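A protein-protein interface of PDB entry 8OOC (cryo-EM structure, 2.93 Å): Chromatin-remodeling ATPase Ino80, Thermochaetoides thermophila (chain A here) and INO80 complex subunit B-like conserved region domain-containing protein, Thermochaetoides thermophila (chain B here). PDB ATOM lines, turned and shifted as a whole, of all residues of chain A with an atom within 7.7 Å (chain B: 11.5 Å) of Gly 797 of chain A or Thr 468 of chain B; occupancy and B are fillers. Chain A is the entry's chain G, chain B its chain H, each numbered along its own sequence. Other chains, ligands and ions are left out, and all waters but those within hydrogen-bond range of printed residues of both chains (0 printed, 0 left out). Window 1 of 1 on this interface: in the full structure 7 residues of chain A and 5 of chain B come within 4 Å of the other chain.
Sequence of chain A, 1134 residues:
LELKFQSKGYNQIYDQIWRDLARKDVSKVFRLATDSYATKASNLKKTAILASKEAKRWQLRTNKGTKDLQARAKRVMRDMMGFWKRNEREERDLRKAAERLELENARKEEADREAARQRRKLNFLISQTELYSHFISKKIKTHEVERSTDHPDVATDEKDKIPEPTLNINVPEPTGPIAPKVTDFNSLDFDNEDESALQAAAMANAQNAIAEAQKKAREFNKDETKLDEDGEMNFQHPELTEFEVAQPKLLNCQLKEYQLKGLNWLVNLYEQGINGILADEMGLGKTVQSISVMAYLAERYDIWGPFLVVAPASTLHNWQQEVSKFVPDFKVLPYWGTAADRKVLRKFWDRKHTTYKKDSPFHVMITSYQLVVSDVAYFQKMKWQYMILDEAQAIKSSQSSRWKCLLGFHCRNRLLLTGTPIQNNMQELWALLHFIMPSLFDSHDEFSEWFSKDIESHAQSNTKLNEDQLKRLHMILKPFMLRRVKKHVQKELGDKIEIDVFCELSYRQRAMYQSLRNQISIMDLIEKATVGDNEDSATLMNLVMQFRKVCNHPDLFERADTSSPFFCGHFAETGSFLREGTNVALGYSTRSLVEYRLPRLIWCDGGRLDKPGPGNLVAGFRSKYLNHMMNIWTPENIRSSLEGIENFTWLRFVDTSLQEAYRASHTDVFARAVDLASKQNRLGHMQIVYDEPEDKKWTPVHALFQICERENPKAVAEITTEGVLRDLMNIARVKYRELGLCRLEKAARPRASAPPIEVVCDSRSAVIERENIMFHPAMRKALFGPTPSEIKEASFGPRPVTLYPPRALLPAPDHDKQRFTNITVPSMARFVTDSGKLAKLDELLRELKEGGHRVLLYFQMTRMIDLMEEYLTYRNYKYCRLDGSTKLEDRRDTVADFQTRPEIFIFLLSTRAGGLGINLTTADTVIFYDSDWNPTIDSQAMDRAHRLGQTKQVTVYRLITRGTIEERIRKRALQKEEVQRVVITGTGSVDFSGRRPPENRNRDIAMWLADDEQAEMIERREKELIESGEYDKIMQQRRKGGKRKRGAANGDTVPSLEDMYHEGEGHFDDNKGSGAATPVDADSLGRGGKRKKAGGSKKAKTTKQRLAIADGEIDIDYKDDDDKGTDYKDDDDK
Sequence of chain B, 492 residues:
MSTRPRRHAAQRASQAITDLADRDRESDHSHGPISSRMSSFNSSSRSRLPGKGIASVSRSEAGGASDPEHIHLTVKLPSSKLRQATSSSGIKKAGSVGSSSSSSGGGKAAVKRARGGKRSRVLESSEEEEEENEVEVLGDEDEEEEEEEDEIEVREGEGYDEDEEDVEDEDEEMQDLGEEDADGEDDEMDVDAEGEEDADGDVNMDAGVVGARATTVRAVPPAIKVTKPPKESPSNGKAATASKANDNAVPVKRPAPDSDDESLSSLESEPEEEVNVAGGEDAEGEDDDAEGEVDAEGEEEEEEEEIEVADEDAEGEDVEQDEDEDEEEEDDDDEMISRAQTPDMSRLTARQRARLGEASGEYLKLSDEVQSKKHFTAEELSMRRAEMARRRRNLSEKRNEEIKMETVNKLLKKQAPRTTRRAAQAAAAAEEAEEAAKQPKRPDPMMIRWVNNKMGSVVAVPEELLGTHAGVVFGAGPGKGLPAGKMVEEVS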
ATOM      1  N   ILE A 791     -23.661   1.676 -40.511  1.00  0.00           N
ATOM      2  CA  ILE A 791     -23.732   2.416 -39.253  1.00  0.00           C
ATOM      3  C   ILE A 791     -24.093   1.491 -38.095  1.00  0.00           C
ATOM      4  O   ILE A 791     -23.543   1.606 -36.993  1.00  0.00           O
ATOM      5  CB  ILE A 791     -24.734   3.579 -39.380  1.00  0.00           C
ATOM      6  CG1 ILE A 791     -24.285   4.550 -40.472  1.00  0.00           C
ATOM      7  CG2 ILE A 791     -24.898   4.296 -38.051  1.00  0.00           C
ATOM      8  CD1 ILE A 791     -25.322   5.594 -40.818  1.00  0.00           C
ATOM      9  N   LYS A 792     -25.021   0.560 -38.326  1.00  0.00           N
ATOM     10  CA  LYS A 792     -25.367  -0.432 -37.310  1.00  0.00           C
ATOM     11  C   LYS A 792     -24.180  -1.324 -36.961  1.00  0.00           C
ATOM     12  O   LYS A 792     -23.854  -1.507 -35.783  1.00  0.00           O
ATOM     13  CB  LYS A 792     -26.558  -1.265 -37.783  1.00  0.00           C
ATOM     14  CG  LYS A 792     -27.850  -0.470 -37.891  1.00  0.00           C
ATOM     15  CD  LYS A 792     -28.922  -1.230 -38.655  1.00  0.00           C
ATOM     16  CE  LYS A 792     -30.126  -0.339 -38.935  1.00  0.00           C
ATOM     17  NZ  LYS A 792     -31.188  -1.039 -39.709  1.00  0.00           N
ATOM     18  N   GLU A 793     -23.529  -1.896 -37.975  1.00  0.00           N
ATOM     19  CA  GLU A 793     -22.351  -2.729 -37.740  1.00  0.00           C
ATOM     20  C   GLU A 793     -21.269  -1.974 -36.976  1.00  0.00           C
ATOM     21  O   GLU A 793     -20.687  -2.499 -36.020  1.00  0.00           O
ATOM     22  CB  GLU A 793     -21.799  -3.244 -39.069  1.00  0.00           C
ATOM     23  CG  GLU A 793     -22.612  -4.356 -39.702  1.00  0.00           C
ATOM     24  CD  GLU A 793     -22.026  -4.824 -41.018  1.00  0.00           C
ATOM     25  OE1 GLU A 793     -20.968  -4.295 -41.418  1.00  0.00           O
ATOM     26  OE2 GLU A 793     -22.618  -5.725 -41.648  1.00  0.00           O
ATOM     27  N   ALA A 794     -20.983  -0.740 -37.388  1.00  0.00           N
ATOM     28  CA  ALA A 794     -19.952   0.055 -36.729  1.00  0.00           C
ATOM     29  C   ALA A 794     -20.315   0.408 -35.289  1.00  0.00           C
ATOM     30  O   ALA A 794     -19.434   0.448 -34.422  1.00  0.00           O
ATOM     31  CB  ALA A 794     -19.686   1.327 -37.532  1.00  0.00           C
ATOM     32  N   SER A 795     -21.593   0.663 -35.004  1.00  0.00           N
ATOM     33  CA  SER A 795     -21.963   1.039 -33.642  1.00  0.00           C
ATOM     34  C   SER A 795     -22.132  -0.154 -32.702  1.00  0.00           C
ATOM     35  O   SER A 795     -21.950   0.002 -31.490  1.00  0.00           O
ATOM     36  CB  SER A 795     -23.250   1.865 -33.663  1.00  0.00           C
ATOM     37  OG  SER A 795     -24.293   1.169 -34.319  1.00  0.00           O
ATOM     38  N   PHE A 796     -22.468  -1.334 -33.215  1.00  0.00           N
ATOM     39  CA  PHE A 796     -22.603  -2.516 -32.370  1.00  0.00           C
ATOM     40  C   PHE A 796     -21.361  -3.395 -32.338  1.00  0.00           C
ATOM     41  O   PHE A 796     -21.357  -4.404 -31.626  1.00  0.00           O
ATOM     42  CB  PHE A 796     -23.815  -3.348 -32.798  1.00  0.00           C
ATOM     43  CG  PHE A 796     -25.118  -2.618 -32.673  1.00  0.00           C
ATOM     44  CD1 PHE A 796     -25.509  -2.087 -31.455  1.00  0.00           C
ATOM     45  CD2 PHE A 796     -25.957  -2.470 -33.763  1.00  0.00           C
ATOM     46  CE1 PHE A 796     -26.707  -1.414 -31.327  1.00  0.00           C
ATOM     47  CE2 PHE A 796     -27.157  -1.797 -33.642  1.00  0.00           C
ATOM     48  CZ  PHE A 796     -27.533  -1.270 -32.422  1.00  0.00           C
ATOM     49  N   GLY A 797     -20.313  -3.050 -33.082  1.00  0.00           N
ATOM     50  CA  GLY A 797     -19.132  -3.876 -33.144  1.00  0.00           C
ATOM     51  C   GLY A 797     -18.418  -3.966 -31.811  1.00  0.00           C
ATOM     52  O   GLY A 797     -18.582  -3.113 -30.932  1.00  0.00           O
ATOM     53  N   PRO A 798     -17.608  -5.013 -31.631  1.00  0.00           N
ATOM     54  CA  PRO A 798     -16.836  -5.125 -30.385  1.00  0.00           C
ATOM     55  C   PRO A 798     -15.680  -4.146 -30.305  1.00  0.00           C
ATOM     56  O   PRO A 798     -15.344  -3.689 -29.206  1.00  0.00           O
ATOM     57  CB  PRO A 798     -16.348  -6.579 -30.412  1.00  0.00           C
ATOM     58  CG  PRO A 798     -16.222  -6.888 -31.866  1.00  0.00           C
ATOM     59  CD  PRO A 798     -17.358  -6.145 -32.539  1.00  0.00           C
ATOM     60  N   ARG A 799     -15.064  -3.812 -31.433  1.00  0.00           N
ATOM     61  CA  ARG A 799     -13.979  -2.852 -31.521  1.00  0.00           C
ATOM     62  C   ARG A 799     -14.326  -1.789 -32.550  1.00  0.00           C
ATOM     63  O   ARG A 799     -15.049  -2.069 -33.512  1.00  0.00           O
ATOM     64  CB  ARG A 799     -12.656  -3.533 -31.900  1.00  0.00           C
ATOM     65  CG  ARG A 799     -12.008  -4.292 -30.755  1.00  0.00           C
ATOM     66  CD  ARG A 799     -10.859  -5.165 -31.237  1.00  0.00           C
ATOM     67  NE  ARG A 799     -10.084  -5.708 -30.128  1.00  0.00           N
ATOM     68  CZ  ARG A 799     -10.501  -6.668 -29.313  1.00  0.00           C
ATOM     69  NH1 ARG A 799     -11.701  -7.208 -29.437  1.00  0.00           N
ATOM     70  NH2 ARG A 799      -9.695  -7.091 -28.344  1.00  0.00           N
ATOM     71  N   PRO A 800     -13.846  -0.558 -32.363  1.00  0.00           N
ATOM     72  CA  PRO A 800     -14.156   0.502 -33.326  1.00  0.00           C
ATOM     73  C   PRO A 800     -13.702   0.137 -34.731  1.00  0.00           C
ATOM     74  O   PRO A 800     -12.727  -0.591 -34.927  1.00  0.00           O
ATOM     75  CB  PRO A 800     -13.382   1.713 -32.787  1.00  0.00           C
ATOM     76  CG  PRO A 800     -13.182   1.420 -31.339  1.00  0.00           C
ATOM     77  CD  PRO A 800     -12.988  -0.067 -31.274  1.00  0.00           C
ATOM     78  N   VAL A 801     -14.429   0.662 -35.713  1.00  0.00           N
ATOM     79  CA  VAL A 801     -14.100   0.500 -37.123  1.00  0.00           C
ATOM     80  C   VAL A 801     -14.292   1.844 -37.813  1.00  0.00           C
ATOM     81  O   VAL A 801     -15.272   2.553 -37.559  1.00  0.00           O
ATOM     82  CB  VAL A 801     -14.940  -0.613 -37.787  1.00  0.00           C
ATOM     83  CG1 VAL A 801     -16.418  -0.272 -37.774  1.00  0.00           C
ATOM     84  CG2 VAL A 801     -14.459  -0.871 -39.206  1.00  0.00           C
ATOM     85  N   ASP B 444     -33.940   3.638 -27.170  1.00  0.00           N
ATOM     86  CA  ASP B 444     -33.366   3.244 -28.448  1.00  0.00           C
ATOM     87  C   ASP B 444     -32.042   2.509 -28.244  1.00  0.00           C
ATOM     88  O   ASP B 444     -31.252   2.878 -27.368  1.00  0.00           O
ATOM     89  CB  ASP B 444     -33.158   4.473 -29.335  1.00  0.00           C
ATOM     90  CG  ASP B 444     -32.470   4.140 -30.645  1.00  0.00           C
ATOM     91  OD1 ASP B 444     -31.222   4.099 -30.673  1.00  0.00           O
ATOM     92  OD2 ASP B 444     -33.177   3.917 -31.649  1.00  0.00           O
ATOM     93  N   PRO B 445     -31.781   1.461 -29.028  1.00  0.00           N
ATOM     94  CA  PRO B 445     -30.535   0.694 -28.871  1.00  0.00           C
ATOM     95  C   PRO B 445     -29.243   1.482 -29.055  1.00  0.00           C
ATOM     96  O   PRO B 445     -28.210   1.050 -28.529  1.00  0.00           O
ATOM     97  CB  PRO B 445     -30.670  -0.391 -29.948  1.00  0.00           C
ATOM     98  CG  PRO B 445     -32.133  -0.631 -30.012  1.00  0.00           C
ATOM     99  CD  PRO B 445     -32.740   0.752 -29.889  1.00  0.00           C
ATOM    100  N   MET B 446     -29.245   2.604 -29.775  1.00  0.00           N
ATOM    101  CA  MET B 446     -27.985   3.247 -30.134  1.00  0.00           C
ATOM    102  C   MET B 446     -27.932   4.752 -29.906  1.00  0.00           C
ATOM    103  O   MET B 446     -26.864   5.341 -30.102  1.00  0.00           O
ATOM    104  CB  MET B 446     -27.646   2.970 -31.606  1.00  0.00           C
ATOM    105  CG  MET B 446     -28.613   3.599 -32.590  1.00  0.00           C
ATOM    106  SD  MET B 446     -27.958   3.672 -34.269  1.00  0.00           S
ATOM    107  CE  MET B 446     -27.769   1.931 -34.644  1.00  0.00           C
ATOM    108  N   MET B 447     -29.025   5.389 -29.505  1.00  0.00           N
ATOM    109  CA  MET B 447     -28.982   6.775 -29.051  1.00  0.00           C
ATOM    110  C   MET B 447     -28.487   6.815 -27.611  1.00  0.00           C
ATOM    111  O   MET B 447     -29.220   6.454 -26.686  1.00  0.00           O
ATOM    112  CB  MET B 447     -30.357   7.423 -29.179  1.00  0.00           C
ATOM    113  CG  MET B 447     -30.773   7.728 -30.609  1.00  0.00           C
ATOM    114  SD  MET B 447     -29.918   9.167 -31.278  1.00  0.00           S
ATOM    115  CE  MET B 447     -30.608   9.241 -32.928  1.00  0.00           C
ATOM    116  N   ILE B 448     -27.246   7.256 -27.416  1.00  0.00           N
ATOM    117  CA  ILE B 448     -26.783   7.630 -26.085  1.00  0.00           C
ATOM    118  C   ILE B 448     -27.384   8.983 -25.734  1.00  0.00           C
ATOM    119  O   ILE B 448     -27.465   9.882 -26.578  1.00  0.00           O
ATOM    120  CB  ILE B 448     -25.245   7.658 -26.037  1.00  0.00           C
ATOM    121  CG1 ILE B 448     -24.683   6.250 -26.215  1.00  0.00           C
ATOM    122  CG2 ILE B 448     -24.760   8.219 -24.722  1.00  0.00           C
ATOM    123  CD1 ILE B 448     -23.173   6.184 -26.158  1.00  0.00           C
ATOM    124  N   ALA B 460     -26.552   8.560 -20.047  1.00  0.00           N
ATOM    125  CA  ALA B 460     -27.120   7.225 -19.919  1.00  0.00           C
ATOM    126  C   ALA B 460     -26.910   6.454 -21.214  1.00  0.00           C
ATOM    127  O   ALA B 460     -27.043   7.015 -22.306  1.00  0.00           O
ATOM    128  CB  ALA B 460     -28.610   7.291 -19.583  1.00  0.00           C
ATOM    129  N   VAL B 461     -26.587   5.170 -21.092  1.00  0.00           N
ATOM    130  CA  VAL B 461     -26.119   4.359 -22.208  1.00  0.00           C
ATOM    131  C   VAL B 461     -27.088   3.200 -22.401  1.00  0.00           C
ATOM    132  O   VAL B 461     -27.440   2.533 -21.426  1.00  0.00           O
ATOM    133  CB  VAL B 461     -24.694   3.823 -21.982  1.00  0.00           C
ATOM    134  CG1 VAL B 461     -24.206   3.064 -23.205  1.00  0.00           C
ATOM    135  CG2 VAL B 461     -23.759   4.957 -21.643  1.00  0.00           C
ATOM    136  N   PRO B 462     -27.552   2.942 -23.622  1.00  0.00           N
ATOM    137  CA  PRO B 462     -28.443   1.799 -23.857  1.00  0.00           C
ATOM    138  C   PRO B 462     -27.787   0.476 -23.485  1.00  0.00           C
ATOM    139  O   PRO B 462     -26.584   0.283 -23.671  1.00  0.00           O
ATOM    140  CB  PRO B 462     -28.731   1.875 -25.362  1.00  0.00           C
ATOM    141  CG  PRO B 462     -28.475   3.290 -25.728  1.00  0.00           C
ATOM    142  CD  PRO B 462     -27.355   3.743 -24.839  1.00  0.00           C
ATOM    143  N   GLU B 463     -28.599  -0.436 -22.942  1.00  0.00           N
ATOM    144  CA  GLU B 463     -28.121  -1.772 -22.591  1.00  0.00           C
ATOM    145  C   GLU B 463     -27.525  -2.503 -23.790  1.00  0.00           C
ATOM    146  O   GLU B 463     -26.674  -3.383 -23.619  1.00  0.00           O
ATOM    147  CB  GLU B 463     -29.263  -2.599 -22.000  1.00  0.00           C
ATOM    148  CG  GLU B 463     -29.873  -2.023 -20.735  1.00  0.00           C
ATOM    149  CD  GLU B 463     -30.970  -2.903 -20.166  1.00  0.00           C
ATOM    150  OE1 GLU B 463     -31.735  -3.488 -20.961  1.00  0.00           O
ATOM    151  OE2 GLU B 463     -31.063  -3.012 -18.926  1.00  0.00           O
ATOM    152  N   GLU B 464     -27.960  -2.158 -25.004  1.00  0.00           N
ATOM    153  CA  GLU B 464     -27.400  -2.738 -26.222  1.00  0.00           C
ATOM    154  C   GLU B 464     -25.979  -2.272 -26.518  1.00  0.00           C
ATOM    155  O   GLU B 464     -25.249  -2.980 -27.218  1.00  0.00           O
ATOM    156  CB  GLU B 464     -28.294  -2.427 -27.427  1.00  0.00           C
ATOM    157  CG  GLU B 464     -29.657  -3.104 -27.408  1.00  0.00           C
ATOM    158  CD  GLU B 464     -30.604  -2.509 -26.388  1.00  0.00           C
ATOM    159  OE1 GLU B 464     -30.373  -1.363 -25.950  1.00  0.00           O
ATOM    160  OE2 GLU B 464     -31.579  -3.197 -26.022  1.00  0.00           O
ATOM    161  N   LEU B 465     -25.568  -1.112 -26.011  1.00  0.00           N
ATOM    162  CA  LEU B 465     -24.218  -0.620 -26.262  1.00  0.00           C
ATOM    163  C   LEU B 465     -23.205  -1.072 -25.219  1.00  0.00           C
ATOM    164  O   LEU B 465     -22.006  -1.088 -25.514  1.00  0.00           O
ATOM    165  CB  LEU B 465     -24.221   0.908 -26.348  1.00  0.00           C
ATOM    166  CG  LEU B 465     -25.082   1.486 -27.475  1.00  0.00           C
ATOM    167  CD1 LEU B 465     -24.774   2.954 -27.688  1.00  0.00           C
ATOM    168  CD2 LEU B 465     -24.881   0.703 -28.765  1.00  0.00           C
ATOM    169  N   LEU B 466     -23.649  -1.424 -24.017  1.00  0.00           N
ATOM    170  CA  LEU B 466     -22.778  -2.114 -23.076  1.00  0.00           C
ATOM    171  C   LEU B 466     -22.324  -3.443 -23.668  1.00  0.00           C
ATOM    172  O   LEU B 466     -23.139  -4.225 -24.167  1.00  0.00           O
ATOM    173  CB  LEU B 466     -23.497  -2.338 -21.746  1.00  0.00           C
ATOM    174  CG  LEU B 466     -24.207  -1.115 -21.168  1.00  0.00           C
ATOM    175  CD1 LEU B 466     -24.766  -1.423 -19.791  1.00  0.00           C
ATOM    176  CD2 LEU B 466     -23.254   0.066 -21.111  1.00  0.00           C
ATOM    177  N   GLY B 467     -21.018  -3.698 -23.611  1.00  0.00           N
ATOM    178  CA  GLY B 467     -20.425  -4.821 -24.306  1.00  0.00           C
ATOM    179  C   GLY B 467     -20.036  -4.553 -25.742  1.00  0.00           C
ATOM    180  O   GLY B 467     -19.447  -5.435 -26.381  1.00  0.00           O
ATOM    181  N   THR B 468     -20.341  -3.374 -26.269  1.00  0.00           N
ATOM    182  CA  THR B 468     -19.765  -2.885 -27.511  1.00  0.00           C
ATOM    183  C   THR B 468     -18.568  -1.994 -27.200  1.00  0.00           C
ATOM    184  O   THR B 468     -18.296  -1.656 -26.046  1.00  0.00           O
ATOM    185  CB  THR B 468     -20.805  -2.123 -28.337  1.00  0.00           C
ATOM    186  OG1 THR B 468     -21.012  -0.823 -27.768  1.00  0.00           O
ATOM    187  CG2 THR B 468     -22.119  -2.882 -28.362  1.00  0.00           C
ATOM    188  N   HIS B 469     -17.837  -1.623 -28.253  1.00  0.00           N
ATOM    189  CA  HIS B 469     -16.745  -0.669 -28.084  1.00  0.00           C
ATOM    190  C   HIS B 469     -17.227   0.654 -27.502  1.00  0.00           C
ATOM    191  O   HIS B 469     -16.478   1.325 -26.787  1.00  0.00           O
ATOM    192  CB  HIS B 469     -16.030  -0.449 -29.418  1.00  0.00           C
ATOM    193  CG  HIS B 469     -16.856   0.261 -30.444  1.00  0.00           C
ATOM    194  ND1 HIS B 469     -17.093   1.618 -30.401  1.00  0.00           N
ATOM    195  CD2 HIS B 469     -17.490  -0.196 -31.549  1.00  0.00           C
ATOM    196  CE1 HIS B 469     -17.843   1.964 -31.431  1.00  0.00           C
ATOM    197  NE2 HIS B 469     -18.098   0.882 -32.144  1.00  0.00           N
ATOM    198  N   ALA B 470     -18.467   1.051 -27.798  1.00  0.00           N
ATOM    199  CA  ALA B 470     -19.005   2.295 -27.259  1.00  0.00           C
ATOM    200  C   ALA B 470     -19.209   2.237 -25.750  1.00  0.00           C
ATOM    201  O   ALA B 470     -19.358   3.288 -25.116  1.00  0.00           O
ATOM    202  CB  ALA B 470     -20.325   2.641 -27.949  1.00  0.00           C
ATOM    203  N   GLY B 471     -19.223   1.037 -25.164  1.00  0.00           N
ATOM    204  CA  GLY B 471     -19.235   0.883 -23.719  1.00  0.00           C
ATOM    205  C   GLY B 471     -17.894   1.054 -23.038  1.00  0.00           C
ATOM    206  O   GLY B 471     -17.858   1.252 -21.819  1.00  0.00           O
ATOM    207  N   VAL B 472     -16.793   0.967 -23.789  1.00  0.00           N
ATOM    208  CA  VAL B 472     -15.461   0.964 -23.183  1.00  0.00           C
ATOM    209  C   VAL B 472     -15.222   2.244 -22.390  1.00  0.00           C
ATOM    210  O   VAL B 472     -14.633   2.215 -21.302  1.00  0.00           O
ATOM    211  CB  VAL B 472     -14.384   0.762 -24.267  1.00  0.00           C
ATOM    212  CG1 VAL B 472     -12.991   0.928 -23.678  1.00  0.00           C
ATOM    213  CG2 VAL B 472     -14.531  -0.601 -24.919  1.00  0.00           C
ATOM    214  N   VAL B 473     -15.674   3.384 -22.916  1.00  0.00           N
ATOM    215  CA  VAL B 473     -15.509   4.652 -22.209  1.00  0.00           C
ATOM    216  C   VAL B 473     -16.243   4.642 -20.874  1.00  0.00           C
ATOM    217  O   VAL B 473     -15.820   5.306 -19.919  1.00  0.00           O
ATOM    218  CB  VAL B 473     -15.979   5.816 -23.105  1.00  0.00           C
ATOM    219  CG1 VAL B 473     -15.736   7.155 -22.425  1.00  0.00           C
ATOM    220  CG2 VAL B 473     -15.276   5.763 -24.452  1.00  0.00           C
ATOM    221  N   PHE B 474     -17.335   3.889 -20.775  1.00  0.00           N
ATOM    222  CA  PHE B 474     -18.167   3.865 -19.580  1.00  0.00           C
ATOM    223  C   PHE B 474     -17.789   2.748 -18.617  1.00  0.00           C
ATOM    224  O   PHE B 474     -18.475   2.556 -17.607  1.00  0.00           O
ATOM    225  CB  PHE B 474     -19.642   3.748 -19.971  1.00  0.00           C
ATOM    226  CG  PHE B 474     -20.100   4.822 -20.912  1.00  0.00           C
ATOM    227  CD1 PHE B 474     -20.431   6.078 -20.437  1.00  0.00           C
ATOM    228  CD2 PHE B 474     -20.185   4.582 -22.271  1.00  0.00           C
ATOM    229  CE1 PHE B 474     -20.848   7.073 -21.298  1.00  0.00           C
ATOM    230  CE2 PHE B 474     -20.602   5.575 -23.138  1.00  0.00           C
ATOM    231  CZ  PHE B 474     -20.934   6.821 -22.650  1.00  0.00           C
ATOM    232  N   GLY B 475     -16.717   2.014 -18.902  1.00  0.00           N
ATOM    233  CA  GLY B 475     -16.343   0.870 -18.098  1.00  0.00           C
ATOM    234  C   GLY B 475     -17.090  -0.401 -18.413  1.00  0.00           C
ATOM    235  O   GLY B 475     -17.162  -1.293 -17.562  1.00  0.00           O
ATOM    236  N   ALA B 476     -17.654  -0.514 -19.612  1.00  0.00           N
ATOM    237  CA  ALA B 476     -18.604  -1.567 -19.944  1.00  0.00           C
ATOM    238  C   ALA B 476     -18.371  -2.044 -21.368  1.00  0.00           C
ATOM    239  O   ALA B 476     -19.316  -2.271 -22.131  1.00  0.00           O
ATOM    240  CB  ALA B 476     -20.045  -1.095 -19.756  1.00  0.00           C
ATOM    241  N   GLY B 477     -17.106  -2.203 -21.743  1.00  0.00           N
ATOM    242  CA  GLY B 477     -16.746  -2.772 -23.019  1.00  0.00           C
ATOM    243  C   GLY B 477     -17.067  -4.248 -23.130  1.00  0.00           C
ATOM    244  O   GLY B 477     -17.738  -4.830 -22.273  1.00  0.00           O
ATOM    245  N   PRO B 478     -16.591  -4.884 -24.212  1.00  0.00           N
ATOM    246  CA  PRO B 478     -16.735  -6.321 -24.472  1.00  0.00           C
ATOM    247  C   PRO B 478     -16.302  -7.190 -23.293  1.00  0.00           C
ATOM    248  O   PRO B 478     -15.428  -6.773 -22.534  1.00  0.00           O
ATOM    249  CB  PRO B 478     -15.818  -6.554 -25.680  1.00  0.00           C
ATOM    250  CG  PRO B 478     -15.752  -5.239 -26.361  1.00  0.00           C
ATOM    251  CD  PRO B 478     -15.815  -4.212 -25.267  1.00  0.00           C
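The backbone carbonyl oxygen (O) of Ala 794 of chain A sits at hydrogen-bond distance from a ring nitrogen (NE2) of His 469 of chain B. O of Gly 797 of chain A lies within hydrogen-bond range of N of His 469 of chain B (3.2 Å). The backbone carbonyl oxygen of Pro 798 of chain A sits close to the backbone NH of His 469 of chain B, at 3.4 Å.
The side-chain hydroxyl (OG) of Ser 795 of chain A lies within hydrogen-bond range of the backbone carbonyl oxygen (O) of Ile 791 of chain A (2.8 Å). The backbone carbonyl oxygen (O) of Lys 792 of chain A sits at hydrogen-bond distance from the side-chain hydroxyl (OG) of Ser 795 of chain A, 3.1 Å away. The backbone NH (N) of Met 446 of chain B lies within hydrogen-bond range of the side-chain carboxylate (OD1) of Asp 444 of chain B (2.6 Å). O of Leu 465 of chain B lies within hydrogen-bond range of OG1 of Thr 468 of chain B (2.5 Å). The backbone NH (N) of Ala 470 of chain B sits close to the side-chain hydroxyl (OG1) of Thr 468 of chain B (3.2 Å).
Among the printed residues, pairs that only touch across the chains: Ser 795 of chain A with Met 446 of chain B, Ser 795 of chain A with Thr 468 of chain B, Phe 796 of chain A with Met 446 of chain B, Phe 796 of chain A with Leu 465 of chain B, Phe 796 of chain A with Thr 468 of chain B, Gly 797 of chain A with Thr 468 of chain B, Pro 798 of chain A with Pro 478 of chain B, Arg 799 of chain A with His 469 of chain B and Pro 800 of chain A with His 469 of chain B.
Gly 797 of chain A touches two residues of chain B. Thr 468 of chain B touches just these residues of chain A: Ser 795, Phe 796 and Gly 797. Ala 794 of chain A touches one residue of chain B. Pro 798 of chain A touches just these residues of chain B: His 469 (3.3 Å) and Pro 478 (3.3 Å). Printed residues of chain B within 4 Å of Ser 795 of chain A: Met 446 and Thr 468. Of the printed residues of chain A, Met 446 of chain B touches Ser 795 (3.6 Å) and Phe 796 (3.9 Å).
Of the 11 printed residues of chain A, 7 touch a printed residue of chain B. Hydrophobic or aromatic side chains of chain A that line the printed part of chain B: Phe 796 and Pro 800. Among the printed residues, 12 pairs touch across the chains.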
